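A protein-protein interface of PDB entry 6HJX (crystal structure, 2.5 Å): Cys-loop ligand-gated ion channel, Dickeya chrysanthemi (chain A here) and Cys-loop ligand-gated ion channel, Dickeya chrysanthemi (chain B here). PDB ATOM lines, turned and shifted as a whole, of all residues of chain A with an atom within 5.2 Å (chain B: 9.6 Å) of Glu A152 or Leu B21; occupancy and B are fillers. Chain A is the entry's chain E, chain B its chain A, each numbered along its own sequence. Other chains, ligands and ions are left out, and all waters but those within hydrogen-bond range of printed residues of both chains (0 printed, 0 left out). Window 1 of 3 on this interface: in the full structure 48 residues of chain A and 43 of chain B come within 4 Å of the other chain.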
ATOM      1  N   ILE A 150      19.544  -5.232  23.028  1.00  0.00           N
ATOM      2  CA  ILE A 150      18.299  -5.262  22.261  1.00  0.00           C
ATOM      3  C   ILE A 150      17.345  -6.345  22.736  1.00  0.00           C
ATOM      4  O   ILE A 150      16.168  -6.337  22.350  1.00  0.00           O
ATOM      5  CB  ILE A 150      18.627  -5.453  20.765  1.00  0.00           C
ATOM      6  CG1 ILE A 150      19.520  -4.311  20.267  1.00  0.00           C
ATOM      7  CG2 ILE A 150      17.357  -5.518  19.923  1.00  0.00           C
ATOM      8  CD1 ILE A 150      20.110  -4.541  18.889  1.00  0.00           C
ATOM      9  N   ASP A 151      17.807  -7.267  23.578  1.00  0.00           N
ATOM     10  CA  ASP A 151      17.006  -8.413  23.982  1.00  0.00           C
ATOM     11  C   ASP A 151      16.224  -8.116  25.254  1.00  0.00           C
ATOM     12  O   ASP A 151      16.757  -7.553  26.215  1.00  0.00           O
ATOM     13  CB  ASP A 151      17.899  -9.638  24.184  1.00  0.00           C
ATOM     14  CG  ASP A 151      18.481 -10.150  22.878  1.00  0.00           C
ATOM     15  OD1 ASP A 151      17.769 -10.102  21.852  1.00  0.00           O
ATOM     16  OD2 ASP A 151      19.649 -10.595  22.876  1.00  0.00           O
ATOM     17  N   GLU A 152      14.947  -8.506  25.247  1.00  0.00           N
ATOM     18  CA  GLU A 152      14.077  -8.250  26.388  1.00  0.00           C
ATOM     19  C   GLU A 152      14.592  -8.937  27.646  1.00  0.00           C
ATOM     20  O   GLU A 152      14.493  -8.386  28.748  1.00  0.00           O
ATOM     21  CB  GLU A 152      12.658  -8.716  26.066  1.00  0.00           C
ATOM     22  CG  GLU A 152      11.620  -8.331  27.104  1.00  0.00           C
ATOM     23  CD  GLU A 152      10.215  -8.723  26.689  1.00  0.00           C
ATOM     24  OE1 GLU A 152      10.075  -9.473  25.698  1.00  0.00           O
ATOM     25  OE2 GLU A 152       9.251  -8.280  27.352  1.00  0.00           O
ATOM     26  N   TRP A 153      15.145 -10.138  27.502  1.00  0.00           N
ATOM     27  CA  TRP A 153      15.635 -10.922  28.627  1.00  0.00           C
ATOM     28  C   TRP A 153      17.132 -11.150  28.491  1.00  0.00           C
ATOM     29  O   TRP A 153      17.645 -11.340  27.384  1.00  0.00           O
ATOM     30  CB  TRP A 153      14.912 -12.267  28.713  1.00  0.00           C
ATOM     31  CG  TRP A 153      13.465 -12.134  29.061  1.00  0.00           C
ATOM     32  CD1 TRP A 153      12.416 -12.057  28.193  1.00  0.00           C
ATOM     33  CD2 TRP A 153      12.905 -12.060  30.376  1.00  0.00           C
ATOM     34  NE1 TRP A 153      11.236 -11.939  28.886  1.00  0.00           N
ATOM     35  CE2 TRP A 153      11.510 -11.938  30.228  1.00  0.00           C
ATOM     36  CE3 TRP A 153      13.448 -12.084  31.663  1.00  0.00           C
ATOM     37  CZ2 TRP A 153      10.649 -11.841  31.320  1.00  0.00           C
ATOM     38  CZ3 TRP A 153      12.594 -11.988  32.746  1.00  0.00           C
ATOM     39  CH2 TRP A 153      11.209 -11.869  32.568  1.00  0.00           C
ATOM     40  N   TRP A 154      17.829 -11.130  29.625  1.00  0.00           N
ATOM     41  CA  TRP A 154      19.269 -11.360  29.681  1.00  0.00           C
ATOM     42  C   TRP A 154      19.510 -12.719  30.328  1.00  0.00           C
ATOM     43  O   TRP A 154      19.253 -12.898  31.523  1.00  0.00           O
ATOM     44  CB  TRP A 154      19.971 -10.252  30.464  1.00  0.00           C
ATOM     45  CG  TRP A 154      19.801  -8.876  29.883  1.00  0.00           C
ATOM     46  CD1 TRP A 154      19.412  -8.562  28.613  1.00  0.00           C
ATOM     47  CD2 TRP A 154      20.010  -7.630  30.558  1.00  0.00           C
ATOM     48  NE1 TRP A 154      19.371  -7.197  28.454  1.00  0.00           N
ATOM     49  CE2 TRP A 154      19.733  -6.603  29.635  1.00  0.00           C
ATOM     50  CE3 TRP A 154      20.406  -7.284  31.854  1.00  0.00           C
ATOM     51  CZ2 TRP A 154      19.838  -5.256  29.967  1.00  0.00           C
ATOM     52  CZ3 TRP A 154      20.510  -5.946  32.180  1.00  0.00           C
ATOM     53  CH2 TRP A 154      20.227  -4.948  31.240  1.00  0.00           C
ATOM     54  N   VAL A 191      17.063 -12.786  33.471  1.00  0.00           N
ATOM     55  CA  VAL A 191      16.613 -11.575  34.144  1.00  0.00           C
ATOM     56  C   VAL A 191      16.053 -10.631  33.094  1.00  0.00           C
ATOM     57  O   VAL A 191      16.485 -10.632  31.935  1.00  0.00           O
ATOM     58  CB  VAL A 191      17.747 -10.896  34.943  1.00  0.00           C
ATOM     59  CG1 VAL A 191      18.339 -11.867  35.956  1.00  0.00           C
ATOM     60  CG2 VAL A 191      18.824 -10.376  34.008  1.00  0.00           C
ATOM     61  N   ARG A 192      15.085  -9.819  33.504  1.00  0.00           N
ATOM     62  CA  ARG A 192      14.453  -8.883  32.588  1.00  0.00           C
ATOM     63  C   ARG A 192      15.368  -7.692  32.328  1.00  0.00           C
ATOM     64  O   ARG A 192      16.195  -7.323  33.165  1.00  0.00           O
ATOM     65  CB  ARG A 192      13.116  -8.397  33.150  1.00  0.00           C
ATOM     66  CG  ARG A 192      12.322  -7.513  32.199  1.00  0.00           C
ATOM     67  CD  ARG A 192      11.042  -7.029  32.850  1.00  0.00           C
ATOM     68  NE  ARG A 192      10.253  -8.142  33.368  1.00  0.00           N
ATOM     69  CZ  ARG A 192       9.329  -8.802  32.675  1.00  0.00           C
ATOM     70  NH1 ARG A 192       9.054  -8.465  31.422  1.00  0.00           N
ATOM     71  NH2 ARG A 192       8.675  -9.804  33.244  1.00  0.00           N
ATOM     72  N   ASN A 193      15.217  -7.099  31.146  1.00  0.00           N
ATOM     73  CA  ASN A 193      15.935  -5.881  30.794  1.00  0.00           C
ATOM     74  C   ASN A 193      15.117  -4.684  31.264  1.00  0.00           C
ATOM     75  O   ASN A 193      14.108  -4.340  30.635  1.00  0.00           O
ATOM     76  CB  ASN A 193      16.184  -5.821  29.285  1.00  0.00           C
ATOM     77  CG  ASN A 193      16.887  -4.546  28.856  1.00  0.00           C
ATOM     78  OD1 ASN A 193      17.312  -3.744  29.689  1.00  0.00           O
ATOM     79  ND2 ASN A 193      17.021  -4.357  27.546  1.00  0.00           N
ATOM     80  N   TYR A 197      11.866   0.369  31.221  1.00  0.00           N
ATOM     81  CA  TYR A 197      10.928   0.760  32.265  1.00  0.00           C
ATOM     82  C   TYR A 197      11.492   1.814  33.204  1.00  0.00           C
ATOM     83  O   TYR A 197      10.717   2.560  33.813  1.00  0.00           O
ATOM     84  CB  TYR A 197      10.497  -0.479  33.051  1.00  0.00           C
ATOM     85  CG  TYR A 197       9.993  -1.581  32.150  1.00  0.00           C
ATOM     86  CD1 TYR A 197       8.719  -1.523  31.596  1.00  0.00           C
ATOM     87  CD2 TYR A 197      10.798  -2.667  31.831  1.00  0.00           C
ATOM     88  CE1 TYR A 197       8.258  -2.520  30.760  1.00  0.00           C
ATOM     89  CE2 TYR A 197      10.344  -3.671  30.997  1.00  0.00           C
ATOM     90  CZ  TYR A 197       9.073  -3.592  30.463  1.00  0.00           C
ATOM     91  OH  TYR A 197       8.615  -4.589  29.631  1.00  0.00           O
ATOM     92  N   GLY B  17       3.045  -7.965   8.231  1.00  0.00           N
ATOM     93  CA  GLY B  17       2.704  -8.484   9.544  1.00  0.00           C
ATOM     94  C   GLY B  17       3.868  -8.526  10.505  1.00  0.00           C
ATOM     95  O   GLY B  17       3.991  -9.478  11.286  1.00  0.00           O
ATOM     96  N   VAL B  18       4.733  -7.514  10.466  1.00  0.00           N
ATOM     97  CA  VAL B  18       5.844  -7.450  11.404  1.00  0.00           C
ATOM     98  C   VAL B  18       5.306  -7.445  12.828  1.00  0.00           C
ATOM     99  O   VAL B  18       4.373  -6.703  13.160  1.00  0.00           O
ATOM    100  CB  VAL B  18       6.706  -6.210  11.124  1.00  0.00           C
ATOM    101  CG1 VAL B  18       7.707  -5.980  12.250  1.00  0.00           C
ATOM    102  CG2 VAL B  18       7.432  -6.361   9.795  1.00  0.00           C
ATOM    103  N   ASN B  19       5.888  -8.285  13.675  1.00  0.00           N
ATOM    104  CA  ASN B  19       5.650  -8.256  15.114  1.00  0.00           C
ATOM    105  C   ASN B  19       6.939  -7.760  15.759  1.00  0.00           C
ATOM    106  O   ASN B  19       7.950  -8.472  15.769  1.00  0.00           O
ATOM    107  CB  ASN B  19       5.247  -9.632  15.635  1.00  0.00           C
ATOM    108  CG  ASN B  19       4.885  -9.617  17.105  1.00  0.00           C
ATOM    109  OD1 ASN B  19       5.525  -8.938  17.907  1.00  0.00           O
ATOM    110  ND2 ASN B  19       3.854 -10.372  17.469  1.00  0.00           N
ATOM    111  N   THR B  20       6.905  -6.531  16.280  1.00  0.00           N
ATOM    112  CA  THR B  20       8.125  -5.906  16.779  1.00  0.00           C
ATOM    113  C   THR B  20       8.635  -6.593  18.039  1.00  0.00           C
ATOM    114  O   THR B  20       9.842  -6.814  18.185  1.00  0.00           O
ATOM    115  CB  THR B  20       7.879  -4.421  17.049  1.00  0.00           C
ATOM    116  OG1 THR B  20       6.717  -4.265  17.876  1.00  0.00           O
ATOM    117  CG2 THR B  20       7.677  -3.671  15.742  1.00  0.00           C
ATOM    118  N   LEU B  21       7.734  -6.941  18.960  1.00  0.00           N
ATOM    119  CA  LEU B  21       8.173  -7.500  20.234  1.00  0.00           C
ATOM    120  C   LEU B  21       8.758  -8.895  20.053  1.00  0.00           C
ATOM    121  O   LEU B  21       9.784  -9.228  20.660  1.00  0.00           O
ATOM    122  CB  LEU B  21       7.006  -7.521  21.220  1.00  0.00           C
ATOM    123  CG  LEU B  21       7.332  -7.845  22.682  1.00  0.00           C
ATOM    124  CD1 LEU B  21       8.392  -6.901  23.240  1.00  0.00           C
ATOM    125  CD2 LEU B  21       6.065  -7.772  23.521  1.00  0.00           C
ATOM    126  N   GLU B  22       8.127  -9.723  19.222  1.00  0.00           N
ATOM    127  CA  GLU B  22       8.621 -11.066  18.954  1.00  0.00           C
ATOM    128  C   GLU B  22       9.663 -11.109  17.843  1.00  0.00           C
ATOM    129  O   GLU B  22      10.236 -12.175  17.597  1.00  0.00           O
ATOM    130  CB  GLU B  22       7.456 -11.992  18.589  1.00  0.00           C
ATOM    131  CG  GLU B  22       6.432 -12.157  19.702  1.00  0.00           C
ATOM    132  CD  GLU B  22       5.325 -13.133  19.348  1.00  0.00           C
ATOM    133  OE1 GLU B  22       5.208 -13.508  18.161  1.00  0.00           O
ATOM    134  OE2 GLU B  22       4.570 -13.530  20.262  1.00  0.00           O
ATOM    135  N   GLN B  23       9.917  -9.989  17.174  1.00  0.00           N
ATOM    136  CA  GLN B  23      10.898  -9.916  16.092  1.00  0.00           C
ATOM    137  C   GLN B  23      10.616 -10.970  15.022  1.00  0.00           C
ATOM    138  O   GLN B  23      11.491 -11.740  14.620  1.00  0.00           O
ATOM    139  CB  GLN B  23      12.319 -10.053  16.641  1.00  0.00           C
ATOM    140  CG  GLN B  23      12.671  -9.000  17.685  1.00  0.00           C
ATOM    141  CD  GLN B  23      14.123  -9.053  18.103  1.00  0.00           C
ATOM    142  OE1 GLN B  23      15.018  -9.148  17.268  1.00  0.00           O
ATOM    143  NE2 GLN B  23      14.364  -8.991  19.405  1.00  0.00           N
ATOM    144  N   THR B  24       9.373 -10.987  14.546  1.00  0.00           N
ATOM    145  CA  THR B  24       8.945 -11.912  13.508  1.00  0.00           C
ATOM    146  C   THR B  24       8.231 -11.149  12.401  1.00  0.00           C
ATOM    147  O   THR B  24       7.889  -9.971  12.541  1.00  0.00           O
ATOM    148  CB  THR B  24       8.024 -13.005  14.068  1.00  0.00           C
ATOM    149  OG1 THR B  24       6.850 -12.405  14.633  1.00  0.00           O
ATOM    150  CG2 THR B  24       8.750 -13.827  15.135  1.00  0.00           C
ATOM    151  N   TYR B  25       8.007 -11.845  11.287  1.00  0.00           N
ATOM    152  CA  TYR B  25       7.307 -11.277  10.145  1.00  0.00           C
ATOM    153  C   TYR B  25       6.775 -12.414   9.285  1.00  0.00           C
ATOM    154  O   TYR B  25       7.235 -13.555   9.375  1.00  0.00           O
ATOM    155  CB  TYR B  25       8.221 -10.366   9.322  1.00  0.00           C
ATOM    156  CG  TYR B  25       9.554 -11.000   9.016  1.00  0.00           C
ATOM    157  CD1 TYR B  25      10.580 -10.958   9.942  1.00  0.00           C
ATOM    158  CD2 TYR B  25       9.786 -11.653   7.810  1.00  0.00           C
ATOM    159  CE1 TYR B  25      11.791 -11.534   9.687  1.00  0.00           C
ATOM    160  CE2 TYR B  25      11.011 -12.239   7.543  1.00  0.00           C
ATOM    161  CZ  TYR B  25      12.011 -12.175   8.495  1.00  0.00           C
ATOM    162  OH  TYR B  25      13.246 -12.746   8.279  1.00  0.00           O
ATOM    163  N   SER B 103      11.382 -15.441  11.916  1.00  0.00           N
ATOM    164  CA  SER B 103      12.043 -14.631  12.926  1.00  0.00           C
ATOM    165  C   SER B 103      13.385 -14.128  12.408  1.00  0.00           C
ATOM    166  O   SER B 103      13.970 -14.681  11.474  1.00  0.00           O
ATOM    167  CB  SER B 103      12.257 -15.432  14.210  1.00  0.00           C
ATOM    168  OG  SER B 103      13.184 -16.479  13.990  1.00  0.00           O
ATOM    169  N   ASN B 104      13.877 -13.073  13.048  1.00  0.00           N
ATOM    170  CA  ASN B 104      15.149 -12.471  12.666  1.00  0.00           C
ATOM    171  C   ASN B 104      15.548 -11.489  13.755  1.00  0.00           C
ATOM    172  O   ASN B 104      14.812 -11.257  14.717  1.00  0.00           O
ATOM    173  CB  ASN B 104      15.066 -11.768  11.307  1.00  0.00           C
ATOM    174  CG  ASN B 104      14.274 -10.479  11.369  1.00  0.00           C
ATOM    175  OD1 ASN B 104      13.305 -10.374  12.121  1.00  0.00           O
ATOM    176  ND2 ASN B 104      14.670  -9.496  10.569  1.00  0.00           N
ATOM    177  N   MET B 106      16.054  -7.871  14.850  1.00  0.00           N
ATOM    178  CA  MET B 106      15.511  -6.583  14.444  1.00  0.00           C
ATOM    179  C   MET B 106      15.771  -5.558  15.533  1.00  0.00           C
ATOM    180  O   MET B 106      15.499  -5.808  16.710  1.00  0.00           O
ATOM    181  CB  MET B 106      14.017  -6.698  14.143  1.00  0.00           C
ATOM    182  CG  MET B 106      13.732  -7.730  13.081  1.00  0.00           C
ATOM    183  SD  MET B 106      12.241  -7.406  12.130  1.00  0.00           S
ATOM    184  CE  MET B 106      10.997  -7.979  13.278  1.00  0.00           C
ATOM    185  N   PHE B 108      14.752  -1.816  16.404  1.00  0.00           N
ATOM    186  CA  PHE B 108      13.844  -0.713  16.115  1.00  0.00           C
ATOM    187  C   PHE B 108      14.228   0.570  16.849  1.00  0.00           C
ATOM    188  O   PHE B 108      13.421   1.501  16.917  1.00  0.00           O
ATOM    189  CB  PHE B 108      12.408  -1.110  16.469  1.00  0.00           C
ATOM    190  CG  PHE B 108      11.931  -2.352  15.767  1.00  0.00           C
ATOM    191  CD1 PHE B 108      11.475  -2.297  14.461  1.00  0.00           C
ATOM    192  CD2 PHE B 108      11.939  -3.575  16.415  1.00  0.00           C
ATOM    193  CE1 PHE B 108      11.040  -3.439  13.810  1.00  0.00           C
ATOM    194  CE2 PHE B 108      11.504  -4.721  15.773  1.00  0.00           C
ATOM    195  CZ  PHE B 108      11.054  -4.654  14.468  1.00  0.00           C
ATOM    196  N   ARG B 191      11.836   1.689   6.635  1.00  0.00           N
ATOM    197  CA  ARG B 191      10.460   2.020   6.975  1.00  0.00           C
ATOM    198  C   ARG B 191      10.051   3.327   6.309  1.00  0.00           C
ATOM    199  O   ARG B 191      10.861   4.246   6.157  1.00  0.00           O
ATOM    200  CB  ARG B 191      10.291   2.133   8.491  1.00  0.00           C
ATOM    201  CG  ARG B 191       8.840   2.306   8.939  1.00  0.00           C
ATOM    202  CD  ARG B 191       8.729   2.545  10.437  1.00  0.00           C
ATOM    203  NE  ARG B 191       9.420   1.516  11.210  1.00  0.00           N
ATOM    204  CZ  ARG B 191       8.891   0.347  11.555  1.00  0.00           C
ATOM    205  NH1 ARG B 191       7.652   0.038  11.200  1.00  0.00           N
ATOM    206  NH2 ARG B 191       9.606  -0.517  12.261  1.00  0.00           N
ATOM    207  N   LEU B 245       2.186   3.233  18.506  1.00  0.00           N
ATOM    208  CA  LEU B 245       3.550   2.801  18.254  1.00  0.00           C
ATOM    209  C   LEU B 245       3.772   1.370  18.743  1.00  0.00           C
ATOM    210  O   LEU B 245       3.043   0.875  19.604  1.00  0.00           O
ATOM    211  CB  LEU B 245       4.533   3.750  18.930  1.00  0.00           C
ATOM    212  CG  LEU B 245       4.433   5.222  18.517  1.00  0.00           C
ATOM    213  CD1 LEU B 245       5.700   5.961  18.912  1.00  0.00           C
ATOM    214  CD2 LEU B 245       4.155   5.390  17.024  1.00  0.00           C
ATOM    215  N   PRO B 246       4.779   0.686  18.204  1.00  0.00           N
ATOM    216  CA  PRO B 246       4.975  -0.728  18.538  1.00  0.00           C
ATOM    217  C   PRO B 246       5.575  -0.941  19.917  1.00  0.00           C
ATOM    218  O   PRO B 246       6.316  -0.107  20.443  1.00  0.00           O
ATOM    219  CB  PRO B 246       5.937  -1.215  17.446  1.00  0.00           C
ATOM    220  CG  PRO B 246       6.699  -0.003  17.057  1.00  0.00           C
ATOM    221  CD  PRO B 246       5.743   1.152  17.188  1.00  0.00           C
ATOM    222  N   ARG B 247       5.242  -2.092  20.497  1.00  0.00           N
ATOM    223  CA  ARG B 247       5.794  -2.498  21.781  1.00  0.00           C
ATOM    224  C   ARG B 247       7.233  -2.963  21.599  1.00  0.00           C
ATOM    225  O   ARG B 247       7.528  -3.767  20.709  1.00  0.00           O
ATOM    226  CB  ARG B 247       4.957  -3.621  22.392  1.00  0.00           C
ATOM    227  CG  ARG B 247       3.502  -3.266  22.608  1.00  0.00           C
ATOM    228  CD  ARG B 247       3.302  -2.461  23.880  1.00  0.00           C
ATOM    229  NE  ARG B 247       1.887  -2.192  24.110  1.00  0.00           N
ATOM    230  CZ  ARG B 247       1.216  -1.178  23.569  1.00  0.00           C
ATOM    231  NH1 ARG B 247       1.830  -0.318  22.765  1.00  0.00           N
ATOM    232  NH2 ARG B 247      -0.072  -1.021  23.838  1.00  0.00           N
ATOM    233  N   LEU B 248       8.121  -2.466  22.447  1.00  0.00           N
ATOM    234  CA  LEU B 248       9.533  -2.803  22.390  1.00  0.00           C
ATOM    235  C   LEU B 248      10.066  -2.932  23.807  1.00  0.00           C
ATOM    236  O   LEU B 248       9.478  -2.387  24.749  1.00  0.00           O
ATOM    237  CB  LEU B 248      10.329  -1.742  21.619  1.00  0.00           C
ATOM    238  CG  LEU B 248       9.925  -1.533  20.155  1.00  0.00           C
ATOM    239  CD1 LEU B 248      10.587  -0.287  19.591  1.00  0.00           C
ATOM    240  CD2 LEU B 248      10.282  -2.752  19.304  1.00  0.00           C
ATOM    241  N   PRO B 249      11.169  -3.656  23.993  1.00  0.00           N
ATOM    242  CA  PRO B 249      11.771  -3.745  25.329  1.00  0.00           C
ATOM    243  C   PRO B 249      12.808  -2.659  25.578  1.00  0.00           C
ATOM    244  O   PRO B 249      13.624  -2.773  26.499  1.00  0.00           O
ATOM    245  CB  PRO B 249      12.412  -5.136  25.320  1.00  0.00           C
ATOM    246  CG  PRO B 249      12.823  -5.327  23.893  1.00  0.00           C
ATOM    247  CD  PRO B 249      11.812  -4.582  23.041  1.00  0.00           C
ATOM    248  N   TYR B 250      12.787  -1.605  24.765  1.00  0.00           N
ATOM    249  CA  TYR B 250      13.776  -0.542  24.867  1.00  0.00           C
ATOM    250  C   TYR B 250      13.178   0.744  24.317  1.00  0.00           C
ATOM    251  O   TYR B 250      12.112   0.745  23.699  1.00  0.00           O
ATOM    252  CB  TYR B 250      15.066  -0.907  24.123  1.00  0.00           C
ATOM    253  CG  TYR B 250      14.851  -1.459  22.732  1.00  0.00           C
ATOM    254  CD1 TYR B 250      14.534  -0.623  21.671  1.00  0.00           C
ATOM    255  CD2 TYR B 250      14.979  -2.817  22.479  1.00  0.00           C
ATOM    256  CE1 TYR B 250      14.342  -1.124  20.400  1.00  0.00           C
ATOM    257  CE2 TYR B 250      14.790  -3.327  21.210  1.00  0.00           C
ATOM    258  CZ  TYR B 250      14.472  -2.474  20.174  1.00  0.00           C
ATOM    259  OH  TYR B 250      14.282  -2.969  18.906  1.00  0.00           O
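The side-chain amide oxygen of Asn B19 sits at hydrogen-bond distance from the backbone NH of Leu B21 (3.2 Å).
OE1 of Gln B23 sits at hydrogen-bond distance from N of Met B106 (2.9 Å).
The side-chain amide oxygen (OD1) of Asn B104 lies close to the side-chain sulfur (SD) of Met B106, 3.2 Å away.
OH of Tyr B250 sits at hydrogen-bond distance from N of Phe B108, at 2.8 Å.
The side-chain amide nitrogen of Asn A193 sits at hydrogen-bond distance from the backbone carbonyl oxygen of Asp A151, at 3.5 Å.
The backbone carbonyl oxygen of Glu A152 lies within hydrogen-bond range of the backbone NH of Asn A193 (2.8 Å).
CG2 of Ile A150 touches O of Met B106, at 3.7 Å.
Pro B249 touches Ile A150.
O of Ile A150 touches CE2 of Tyr B250 (3.5 Å).
Glu A152 touches Leu B21.
Glu A152 touches Pro B249 (CB to CB, 3.7 Å).
Pro B249 touches Asn A193 (O to ND2, 3.9 Å).
Of chain B, only Leu B21 (3.9 Å) and Pro B249 (3.7 Å) come within 4 Å of Glu A152.
Leu B21 touches one residue of chain A.
Asn A193 touches just one residue of chain B: Pro B249.
Of the printed residues of chain B, Ile A150 touches Met B106, Pro B249 and Tyr B250.
Of the printed residues of chain A, Met B106 touches Ile A150.
Trp A153 touches none of the printed residues of chain B.
Arg A192 touches none of the printed residues of chain B.
The nearest printed residue of chain A that does not touch Leu B21 is Tyr A197 (6.8 Å).
The nearest printed residue of chain A that does not touch Met B106 is Asp A151 (7.1 Å).
Hydrophobic or aromatic side chains of chain A within 4 Å of the printed part of chain B: Ile A150.
Of the 20 printed residues of chain B, 4 touch a printed residue of chain A.
Hydrophobic or aromatic side chains of chain B that line the printed part of chain A: Leu B21, Pro B249 and Tyr B250.
Among the printed residues, no Asp or Glu carboxylate lies within 4 Å of a Lys or Arg side-chain nitrogen of the other chain.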
